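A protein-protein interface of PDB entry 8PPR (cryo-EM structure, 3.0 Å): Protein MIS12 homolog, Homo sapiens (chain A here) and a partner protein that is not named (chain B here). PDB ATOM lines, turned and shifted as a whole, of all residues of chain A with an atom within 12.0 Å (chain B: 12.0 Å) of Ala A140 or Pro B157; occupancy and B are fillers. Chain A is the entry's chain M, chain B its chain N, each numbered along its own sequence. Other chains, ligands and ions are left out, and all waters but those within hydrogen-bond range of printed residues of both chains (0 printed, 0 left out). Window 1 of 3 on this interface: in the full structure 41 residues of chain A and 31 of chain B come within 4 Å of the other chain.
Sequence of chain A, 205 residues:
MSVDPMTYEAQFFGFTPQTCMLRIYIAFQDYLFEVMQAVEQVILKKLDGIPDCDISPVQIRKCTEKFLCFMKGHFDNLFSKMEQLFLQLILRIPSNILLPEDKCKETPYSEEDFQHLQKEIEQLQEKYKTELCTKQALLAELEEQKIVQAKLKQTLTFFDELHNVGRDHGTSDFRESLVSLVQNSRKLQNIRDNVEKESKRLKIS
OE2 of Glu A144 lies within hydrogen-bond range of N of Leu B158, 2.7 Å away.
Pro B153 touches Leu A132.
Pro B153 touches Cys A133.
Pro B153 touches Gln A136.
Val B155 touches Gln A136.
Ala A137 touches Val B155.
Ala A140 touches Val B155 (CB to O, 3.8 Å).
Pro B157 touches Ala A140.
CA of Pro B157 touches OE2 of Glu A144 (3.3 Å).
Ile A147 touches Leu B160 (CG2 to CD1, 3.6 Å).
Tyr B162 touches Ile A147 (OH to CG2, 3.1 Å).
Of the printed residues of chain B, Cys A133 touches Pro B153 (3.7 Å).
Ala A137 touches one residue of chain B.
No residue of chain B comes within 4 Å of Leu A139.
Ala A140 touches two residues of chain B.
No residue of chain B comes within 4 Å of Glu A141.
Leu A142 touches none of the printed residues of chain B.
No residue of chain B comes within 4 Å of Glu A143.
Of chain B, only Pro B157 (3.3 Å) and Leu B158 (2.7 Å) come within 4 Å of Glu A144.
Gln A145 touches none of the printed residues of chain B.
Val B155 touches just these residues of chain A: Gln A136, Ala A137 and Ala A140.
No residue of chain A comes within 4 Å of His B156.
Printed residues of chain A within 4 Å of Pro B157: Ala A140 (3.8 Å) and Glu A144 (3.3 Å).
Leu B158 touches just one residue of chain A: Glu A144 (2.7 Å).
No residue of chain A comes within 4 Å of Asp B159.
Of the printed residues of chain A, Tyr B162 touches Ile A147 (3.1 Å).
The nearest residue of chain A that does not touch Pro B157 is Glu A143 (4.6 Å).
Of the 19 printed residues of chain A, 7 touch a printed residue of chain B.
Printed residues of chain A that touch a printed residue of chain B: Leu A132, Cys A133, Gln A136, Ala A137, Ala A140, Glu A144 and Ile A147.
Hydrophobic or aromatic side chains of chain A that line the printed part of chain B: Leu A132, Ala A140 and Ile A147.
Hydrophobic or aromatic side chains of chain B that line the printed part of chain A: Pro B153, Val B155, Pro B157, Leu B158, Leu B160 and Tyr B162.
Among the printed residues, no Asp or Glu carboxylate lies within 4 Å of a Lys or Arg side-chain nitrogen of the other chain.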
ATOM      1  N   GLU A 131      30.399  13.000 -28.778  1.00  0.00           N
ATOM      2  CA  GLU A 131      30.571  12.003 -29.829  1.00  0.00           C
ATOM      3  C   GLU A 131      31.388  10.812 -29.345  1.00  0.00           C
ATOM      4  O   GLU A 131      31.111   9.669 -29.726  1.00  0.00           O
ATOM      5  CB  GLU A 131      31.220  12.637 -31.058  1.00  0.00           C
ATOM      6  CG  GLU A 131      30.422  13.772 -31.669  1.00  0.00           C
ATOM      7  CD  GLU A 131      29.175  13.288 -32.381  1.00  0.00           C
ATOM      8  OE1 GLU A 131      29.054  12.066 -32.616  1.00  0.00           O
ATOM      9  OE2 GLU A 131      28.312  14.129 -32.707  1.00  0.00           O
ATOM     10  N   LEU A 132      32.408  11.057 -28.517  1.00  0.00           N
ATOM     11  CA  LEU A 132      33.173   9.942 -27.963  1.00  0.00           C
ATOM     12  C   LEU A 132      32.285   9.031 -27.123  1.00  0.00           C
ATOM     13  O   LEU A 132      32.333   7.797 -27.253  1.00  0.00           O
ATOM     14  CB  LEU A 132      34.337  10.473 -27.128  1.00  0.00           C
ATOM     15  CG  LEU A 132      35.556  10.962 -27.909  1.00  0.00           C
ATOM     16  CD1 LEU A 132      36.539  11.664 -26.985  1.00  0.00           C
ATOM     17  CD2 LEU A 132      36.226   9.803 -28.628  1.00  0.00           C
ATOM     18  N   CYS A 133      31.453   9.627 -26.267  1.00  0.00           N
ATOM     19  CA  CYS A 133      30.538   8.838 -25.451  1.00  0.00           C
ATOM     20  C   CYS A 133      29.547   8.077 -26.324  1.00  0.00           C
ATOM     21  O   CYS A 133      29.222   6.915 -26.045  1.00  0.00           O
ATOM     22  CB  CYS A 133      29.804   9.749 -24.471  1.00  0.00           C
ATOM     23  SG  CYS A 133      30.871  10.488 -23.214  1.00  0.00           S
ATOM     24  N   THR A 134      29.051   8.725 -27.379  1.00  0.00           N
ATOM     25  CA  THR A 134      28.128   8.062 -28.293  1.00  0.00           C
ATOM     26  C   THR A 134      28.780   6.857 -28.953  1.00  0.00           C
ATOM     27  O   THR A 134      28.162   5.795 -29.075  1.00  0.00           O
ATOM     28  CB  THR A 134      27.648   9.051 -29.352  1.00  0.00           C
ATOM     29  OG1 THR A 134      27.014  10.163 -28.711  1.00  0.00           O
ATOM     30  CG2 THR A 134      26.663   8.382 -30.298  1.00  0.00           C
ATOM     31  N   LYS A 135      30.032   7.006 -29.386  1.00  0.00           N
ATOM     32  CA  LYS A 135      30.746   5.886 -29.986  1.00  0.00           C
ATOM     33  C   LYS A 135      30.900   4.741 -28.995  1.00  0.00           C
ATOM     34  O   LYS A 135      30.720   3.569 -29.351  1.00  0.00           O
ATOM     35  CB  LYS A 135      32.110   6.351 -30.493  1.00  0.00           C
ATOM     36  CG  LYS A 135      33.176   5.272 -30.495  1.00  0.00           C
ATOM     37  CD  LYS A 135      34.515   5.824 -30.944  1.00  0.00           C
ATOM     38  CE  LYS A 135      35.622   4.800 -30.761  1.00  0.00           C
ATOM     39  NZ  LYS A 135      36.912   5.272 -31.334  1.00  0.00           N
ATOM     40  N   GLN A 136      31.232   5.060 -27.741  1.00  0.00           N
ATOM     41  CA  GLN A 136      31.358   4.009 -26.734  1.00  0.00           C
ATOM     42  C   GLN A 136      30.037   3.272 -26.536  1.00  0.00           C
ATOM     43  O   GLN A 136      30.002   2.033 -26.472  1.00  0.00           O
ATOM     44  CB  GLN A 136      31.839   4.610 -25.414  1.00  0.00           C
ATOM     45  CG  GLN A 136      33.318   4.945 -25.392  1.00  0.00           C
ATOM     46  CD  GLN A 136      34.170   3.846 -25.989  1.00  0.00           C
ATOM     47  OE1 GLN A 136      34.123   2.698 -25.548  1.00  0.00           O
ATOM     48  NE2 GLN A 136      34.955   4.193 -27.002  1.00  0.00           N
ATOM     49  N   ALA A 137      28.935   4.021 -26.456  1.00  0.00           N
ATOM     50  CA  ALA A 137      27.628   3.397 -26.296  1.00  0.00           C
ATOM     51  C   ALA A 137      27.286   2.523 -27.496  1.00  0.00           C
ATOM     52  O   ALA A 137      26.691   1.450 -27.346  1.00  0.00           O
ATOM     53  CB  ALA A 137      26.557   4.467 -26.086  1.00  0.00           C
ATOM     54  N   LEU A 138      27.656   2.968 -28.697  1.00  0.00           N
ATOM     55  CA  LEU A 138      27.384   2.176 -29.890  1.00  0.00           C
ATOM     56  C   LEU A 138      28.186   0.881 -29.892  1.00  0.00           C
ATOM     57  O   LEU A 138      27.674  -0.169 -30.295  1.00  0.00           O
ATOM     58  CB  LEU A 138      27.668   3.004 -31.142  1.00  0.00           C
ATOM     59  CG  LEU A 138      26.690   4.168 -31.334  1.00  0.00           C
ATOM     60  CD1 LEU A 138      26.754   4.734 -32.738  1.00  0.00           C
ATOM     61  CD2 LEU A 138      25.271   3.732 -31.000  1.00  0.00           C
ATOM     62  N   LEU A 139      29.443   0.929 -29.445  1.00  0.00           N
ATOM     63  CA  LEU A 139      30.212  -0.306 -29.309  1.00  0.00           C
ATOM     64  C   LEU A 139      29.554  -1.260 -28.320  1.00  0.00           C
ATOM     65  O   LEU A 139      29.474  -2.474 -28.566  1.00  0.00           O
ATOM     66  CB  LEU A 139      31.648  -0.003 -28.880  1.00  0.00           C
ATOM     67  CG  LEU A 139      32.698   0.182 -29.979  1.00  0.00           C
ATOM     68  CD1 LEU A 139      32.512   1.480 -30.736  1.00  0.00           C
ATOM     69  CD2 LEU A 139      34.096   0.108 -29.383  1.00  0.00           C
ATOM     70  N   ALA A 140      29.073  -0.729 -27.194  1.00  0.00           N
ATOM     71  CA  ALA A 140      28.365  -1.574 -26.236  1.00  0.00           C
ATOM     72  C   ALA A 140      27.129  -2.205 -26.869  1.00  0.00           C
ATOM     73  O   ALA A 140      26.839  -3.391 -26.651  1.00  0.00           O
ATOM     74  CB  ALA A 140      27.982  -0.761 -25.000  1.00  0.00           C
ATOM     75  N   GLU A 141      26.390  -1.424 -27.659  1.00  0.00           N
ATOM     76  CA  GLU A 141      25.203  -1.951 -28.321  1.00  0.00           C
ATOM     77  C   GLU A 141      25.561  -3.044 -29.319  1.00  0.00           C
ATOM     78  O   GLU A 141      24.844  -4.042 -29.434  1.00  0.00           O
ATOM     79  CB  GLU A 141      24.435  -0.827 -29.015  1.00  0.00           C
ATOM     80  CG  GLU A 141      23.063  -1.256 -29.509  1.00  0.00           C
ATOM     81  CD  GLU A 141      22.140  -0.084 -29.768  1.00  0.00           C
ATOM     82  OE1 GLU A 141      22.532   1.062 -29.463  1.00  0.00           O
ATOM     83  OE2 GLU A 141      21.020  -0.309 -30.274  1.00  0.00           O
ATOM     84  N   LEU A 142      26.657  -2.867 -30.063  1.00  0.00           N
ATOM     85  CA  LEU A 142      27.098  -3.922 -30.975  1.00  0.00           C
ATOM     86  C   LEU A 142      27.431  -5.201 -30.222  1.00  0.00           C
ATOM     87  O   LEU A 142      27.084  -6.300 -30.671  1.00  0.00           O
ATOM     88  CB  LEU A 142      28.306  -3.471 -31.797  1.00  0.00           C
ATOM     89  CG  LEU A 142      28.064  -2.831 -33.167  1.00  0.00           C
ATOM     90  CD1 LEU A 142      27.511  -1.434 -33.059  1.00  0.00           C
ATOM     91  CD2 LEU A 142      29.349  -2.836 -33.982  1.00  0.00           C
ATOM     92  N   GLU A 143      28.114  -5.083 -29.083  1.00  0.00           N
ATOM     93  CA  GLU A 143      28.433  -6.280 -28.307  1.00  0.00           C
ATOM     94  C   GLU A 143      27.166  -6.983 -27.831  1.00  0.00           C
ATOM     95  O   GLU A 143      27.047  -8.215 -27.929  1.00  0.00           O
ATOM     96  CB  GLU A 143      29.323  -5.913 -27.121  1.00  0.00           C
ATOM     97  CG  GLU A 143      30.717  -5.469 -27.523  1.00  0.00           C
ATOM     98  CD  GLU A 143      31.497  -6.569 -28.216  1.00  0.00           C
ATOM     99  OE1 GLU A 143      31.299  -7.752 -27.868  1.00  0.00           O
ATOM    100  OE2 GLU A 143      32.306  -6.250 -29.111  1.00  0.00           O
ATOM    101  N   GLU A 144      26.202  -6.212 -27.326  1.00  0.00           N
ATOM    102  CA  GLU A 144      24.951  -6.806 -26.862  1.00  0.00           C
ATOM    103  C   GLU A 144      24.193  -7.462 -28.012  1.00  0.00           C
ATOM    104  O   GLU A 144      23.612  -8.544 -27.850  1.00  0.00           O
ATOM    105  CB  GLU A 144      24.096  -5.740 -26.182  1.00  0.00           C
ATOM    106  CG  GLU A 144      24.671  -5.266 -24.860  1.00  0.00           C
ATOM    107  CD  GLU A 144      24.039  -3.979 -24.381  1.00  0.00           C
ATOM    108  OE1 GLU A 144      23.012  -3.574 -24.963  1.00  0.00           O
ATOM    109  OE2 GLU A 144      24.571  -3.369 -23.431  1.00  0.00           O
ATOM    110  N   GLN A 145      24.191  -6.819 -29.182  1.00  0.00           N
ATOM    111  CA  GLN A 145      23.544  -7.395 -30.353  1.00  0.00           C
ATOM    112  C   GLN A 145      24.208  -8.703 -30.757  1.00  0.00           C
ATOM    113  O   GLN A 145      23.527  -9.664 -31.129  1.00  0.00           O
ATOM    114  CB  GLN A 145      23.583  -6.398 -31.510  1.00  0.00           C
ATOM    115  CG  GLN A 145      22.576  -5.269 -31.393  1.00  0.00           C
ATOM    116  CD  GLN A 145      22.635  -4.316 -32.570  1.00  0.00           C
ATOM    117  OE1 GLN A 145      23.493  -4.444 -33.443  1.00  0.00           O
ATOM    118  NE2 GLN A 145      21.726  -3.351 -32.596  1.00  0.00           N
ATOM    119  N   LYS A 146      25.540  -8.753 -30.698  1.00  0.00           N
ATOM    120  CA  LYS A 146      26.250  -9.991 -30.999  1.00  0.00           C
ATOM    121  C   LYS A 146      25.844 -11.101 -30.043  1.00  0.00           C
ATOM    122  O   LYS A 146      25.614 -12.244 -30.461  1.00  0.00           O
ATOM    123  CB  LYS A 146      27.757  -9.754 -30.926  1.00  0.00           C
ATOM    124  CG  LYS A 146      28.589 -11.013 -31.086  1.00  0.00           C
ATOM    125  CD  LYS A 146      30.004 -10.806 -30.571  1.00  0.00           C
ATOM    126  CE  LYS A 146      30.629  -9.544 -31.143  1.00  0.00           C
ATOM    127  NZ  LYS A 146      30.553  -9.506 -32.630  1.00  0.00           N
ATOM    128  N   ILE A 147      25.751 -10.783 -28.751  1.00  0.00           N
ATOM    129  CA  ILE A 147      25.355 -11.787 -27.764  1.00  0.00           C
ATOM    130  C   ILE A 147      23.948 -12.300 -28.059  1.00  0.00           C
ATOM    131  O   ILE A 147      23.681 -13.513 -28.031  1.00  0.00           O
ATOM    132  CB  ILE A 147      25.457 -11.202 -26.345  1.00  0.00           C
ATOM    133  CG1 ILE A 147      26.914 -10.876 -26.013  1.00  0.00           C
ATOM    134  CG2 ILE A 147      24.870 -12.157 -25.335  1.00  0.00           C
ATOM    135  CD1 ILE A 147      27.828 -12.080 -26.045  1.00  0.00           C
ATOM    136  N   VAL A 148      23.028 -11.378 -28.349  1.00  0.00           N
ATOM    137  CA  VAL A 148      21.648 -11.763 -28.630  1.00  0.00           C
ATOM    138  C   VAL A 148      21.584 -12.643 -29.872  1.00  0.00           C
ATOM    139  O   VAL A 148      20.860 -13.646 -29.907  1.00  0.00           O
ATOM    140  CB  VAL A 148      20.767 -10.507 -28.774  1.00  0.00           C
ATOM    141  CG1 VAL A 148      19.461 -10.844 -29.475  1.00  0.00           C
ATOM    142  CG2 VAL A 148      20.506  -9.886 -27.411  1.00  0.00           C
ATOM    143  N   GLN A 149      22.344 -12.282 -30.909  1.00  0.00           N
ATOM    144  CA  GLN A 149      22.364 -13.079 -32.130  1.00  0.00           C
ATOM    145  C   GLN A 149      22.913 -14.473 -31.869  1.00  0.00           C
ATOM    146  O   GLN A 149      22.424 -15.457 -32.435  1.00  0.00           O
ATOM    147  CB  GLN A 149      23.190 -12.368 -33.199  1.00  0.00           C
ATOM    148  CG  GLN A 149      22.533 -11.117 -33.748  1.00  0.00           C
ATOM    149  CD  GLN A 149      23.131 -10.685 -35.066  1.00  0.00           C
ATOM    150  OE1 GLN A 149      23.925 -11.407 -35.666  1.00  0.00           O
ATOM    151  NE2 GLN A 149      22.759  -9.494 -35.521  1.00  0.00           N
ATOM    152  N   PRO B 153      36.083   7.968 -22.323  1.00  0.00           N
ATOM    153  CA  PRO B 153      34.811   7.548 -21.728  1.00  0.00           C
ATOM    154  C   PRO B 153      34.654   6.037 -21.766  1.00  0.00           C
ATOM    155  O   PRO B 153      35.081   5.360 -22.702  1.00  0.00           O
ATOM    156  CB  PRO B 153      33.775   8.238 -22.623  1.00  0.00           C
ATOM    157  CG  PRO B 153      34.439   8.323 -23.963  1.00  0.00           C
ATOM    158  CD  PRO B 153      35.938   8.346 -23.739  1.00  0.00           C
ATOM    159  N   VAL B 154      34.034   5.502 -20.718  1.00  0.00           N
ATOM    160  CA  VAL B 154      33.822   4.067 -20.573  1.00  0.00           C
ATOM    161  C   VAL B 154      32.327   3.802 -20.479  1.00  0.00           C
ATOM    162  O   VAL B 154      31.622   4.443 -19.691  1.00  0.00           O
ATOM    163  CB  VAL B 154      34.567   3.504 -19.349  1.00  0.00           C
ATOM    164  CG1 VAL B 154      36.062   3.483 -19.612  1.00  0.00           C
ATOM    165  CG2 VAL B 154      34.263   4.331 -18.108  1.00  0.00           C
ATOM    166  N   VAL B 155      31.843   2.871 -21.298  1.00  0.00           N
ATOM    167  CA  VAL B 155      30.442   2.462 -21.306  1.00  0.00           C
ATOM    168  C   VAL B 155      30.432   0.938 -21.321  1.00  0.00           C
ATOM    169  O   VAL B 155      30.572   0.321 -22.383  1.00  0.00           O
ATOM    170  CB  VAL B 155      29.666   3.032 -22.499  1.00  0.00           C
ATOM    171  CG1 VAL B 155      28.237   2.509 -22.502  1.00  0.00           C
ATOM    172  CG2 VAL B 155      29.674   4.554 -22.464  1.00  0.00           C
ATOM    173  N   HIS B 156      30.282   0.330 -20.154  1.00  0.00           N
ATOM    174  CA  HIS B 156      30.187  -1.122 -20.084  1.00  0.00           C
ATOM    175  C   HIS B 156      28.830  -1.572 -20.613  1.00  0.00           C
ATOM    176  O   HIS B 156      27.800  -1.012 -20.218  1.00  0.00           O
ATOM    177  CB  HIS B 156      30.380  -1.614 -18.653  1.00  0.00           C
ATOM    178  CG  HIS B 156      31.502  -0.940 -17.928  1.00  0.00           C
ATOM    179  ND1 HIS B 156      32.793  -1.423 -17.942  1.00  0.00           N
ATOM    180  CD2 HIS B 156      31.526   0.173 -17.158  1.00  0.00           C
ATOM    181  CE1 HIS B 156      33.564  -0.633 -17.218  1.00  0.00           C
ATOM    182  NE2 HIS B 156      32.820   0.343 -16.731  1.00  0.00           N
ATOM    183  N   PRO B 157      28.782  -2.561 -21.503  1.00  0.00           N
ATOM    184  CA  PRO B 157      27.483  -3.071 -21.956  1.00  0.00           C
ATOM    185  C   PRO B 157      26.737  -3.734 -20.811  1.00  0.00           C
ATOM    186  O   PRO B 157      27.339  -4.333 -19.917  1.00  0.00           O
ATOM    187  CB  PRO B 157      27.848  -4.081 -23.050  1.00  0.00           C
ATOM    188  CG  PRO B 157      29.272  -4.433 -22.818  1.00  0.00           C
ATOM    189  CD  PRO B 157      29.919  -3.346 -22.014  1.00  0.00           C
ATOM    190  N   LEU B 158      25.412  -3.613 -20.840  1.00  0.00           N
ATOM    191  CA  LEU B 158      24.595  -4.195 -19.785  1.00  0.00           C
ATOM    192  C   LEU B 158      24.724  -5.713 -19.803  1.00  0.00           C
ATOM    193  O   LEU B 158      24.717  -6.340 -20.866  1.00  0.00           O
ATOM    194  CB  LEU B 158      23.134  -3.765 -19.944  1.00  0.00           C
ATOM    195  CG  LEU B 158      22.350  -4.138 -21.206  1.00  0.00           C
ATOM    196  CD1 LEU B 158      21.618  -5.463 -21.040  1.00  0.00           C
ATOM    197  CD2 LEU B 158      21.377  -3.029 -21.577  1.00  0.00           C
ATOM    198  N   ASP B 159      24.861  -6.300 -18.619  1.00  0.00           N
ATOM    199  CA  ASP B 159      25.096  -7.734 -18.499  1.00  0.00           C
ATOM    200  C   ASP B 159      23.796  -8.488 -18.744  1.00  0.00           C
ATOM    201  O   ASP B 159      22.831  -8.344 -17.987  1.00  0.00           O
ATOM    202  CB  ASP B 159      25.667  -8.055 -17.122  1.00  0.00           C
ATOM    203  CG  ASP B 159      26.890  -7.221 -16.793  1.00  0.00           C
ATOM    204  OD1 ASP B 159      27.584  -6.787 -17.736  1.00  0.00           O
ATOM    205  OD2 ASP B 159      27.154  -6.997 -15.594  1.00  0.00           O
ATOM    206  N   LEU B 160      23.765  -9.289 -19.805  1.00  0.00           N
ATOM    207  CA  LEU B 160      22.607 -10.120 -20.097  1.00  0.00           C
ATOM    208  C   LEU B 160      22.671 -11.399 -19.273  1.00  0.00           C
ATOM    209  O   LEU B 160      23.697 -12.086 -19.255  1.00  0.00           O
ATOM    210  CB  LEU B 160      22.542 -10.440 -21.590  1.00  0.00           C
ATOM    211  CG  LEU B 160      22.406  -9.222 -22.506  1.00  0.00           C
ATOM    212  CD1 LEU B 160      22.836  -9.554 -23.922  1.00  0.00           C
ATOM    213  CD2 LEU B 160      20.977  -8.712 -22.495  1.00  0.00           C
ATOM    214  N   LYS B 161      21.575 -11.717 -18.592  1.00  0.00           N
ATOM    215  CA  LYS B 161      21.547 -12.820 -17.641  1.00  0.00           C
ATOM    216  C   LYS B 161      21.183 -14.122 -18.340  1.00  0.00           C
ATOM    217  O   LYS B 161      20.265 -14.161 -19.166  1.00  0.00           O
ATOM    218  CB  LYS B 161      20.554 -12.538 -16.510  1.00  0.00           C
ATOM    219  CG  LYS B 161      20.409 -11.071 -16.123  1.00  0.00           C
ATOM    220  CD  LYS B 161      21.746 -10.450 -15.741  1.00  0.00           C
ATOM    221  CE  LYS B 161      21.558  -9.084 -15.102  1.00  0.00           C
ATOM    222  NZ  LYS B 161      22.840  -8.542 -14.574  1.00  0.00           N
ATOM    223  N   TYR B 162      21.911 -15.188 -18.002  1.00  0.00           N
ATOM    224  CA  TYR B 162      21.632 -16.535 -18.481  1.00  0.00           C
ATOM    225  C   TYR B 162      21.082 -17.428 -17.378  1.00  0.00           C
ATOM    226  O   TYR B 162      21.318 -18.641 -17.401  1.00  0.00           O
ATOM    227  CB  TYR B 162      22.893 -17.174 -19.061  1.00  0.00           C
ATOM    228  CG  TYR B 162      23.448 -16.513 -20.297  1.00  0.00           C
ATOM    229  CD1 TYR B 162      22.711 -15.577 -21.008  1.00  0.00           C
ATOM    230  CD2 TYR B 162      24.717 -16.834 -20.754  1.00  0.00           C
ATOM    231  CE1 TYR B 162      23.227 -14.978 -22.140  1.00  0.00           C
ATOM    232  CE2 TYR B 162      25.240 -16.245 -21.879  1.00  0.00           C
ATOM    233  CZ  TYR B 162      24.493 -15.319 -22.568  1.00  0.00           C
ATOM    234  OH  TYR B 162      25.026 -14.738 -23.691  1.00  0.00           O
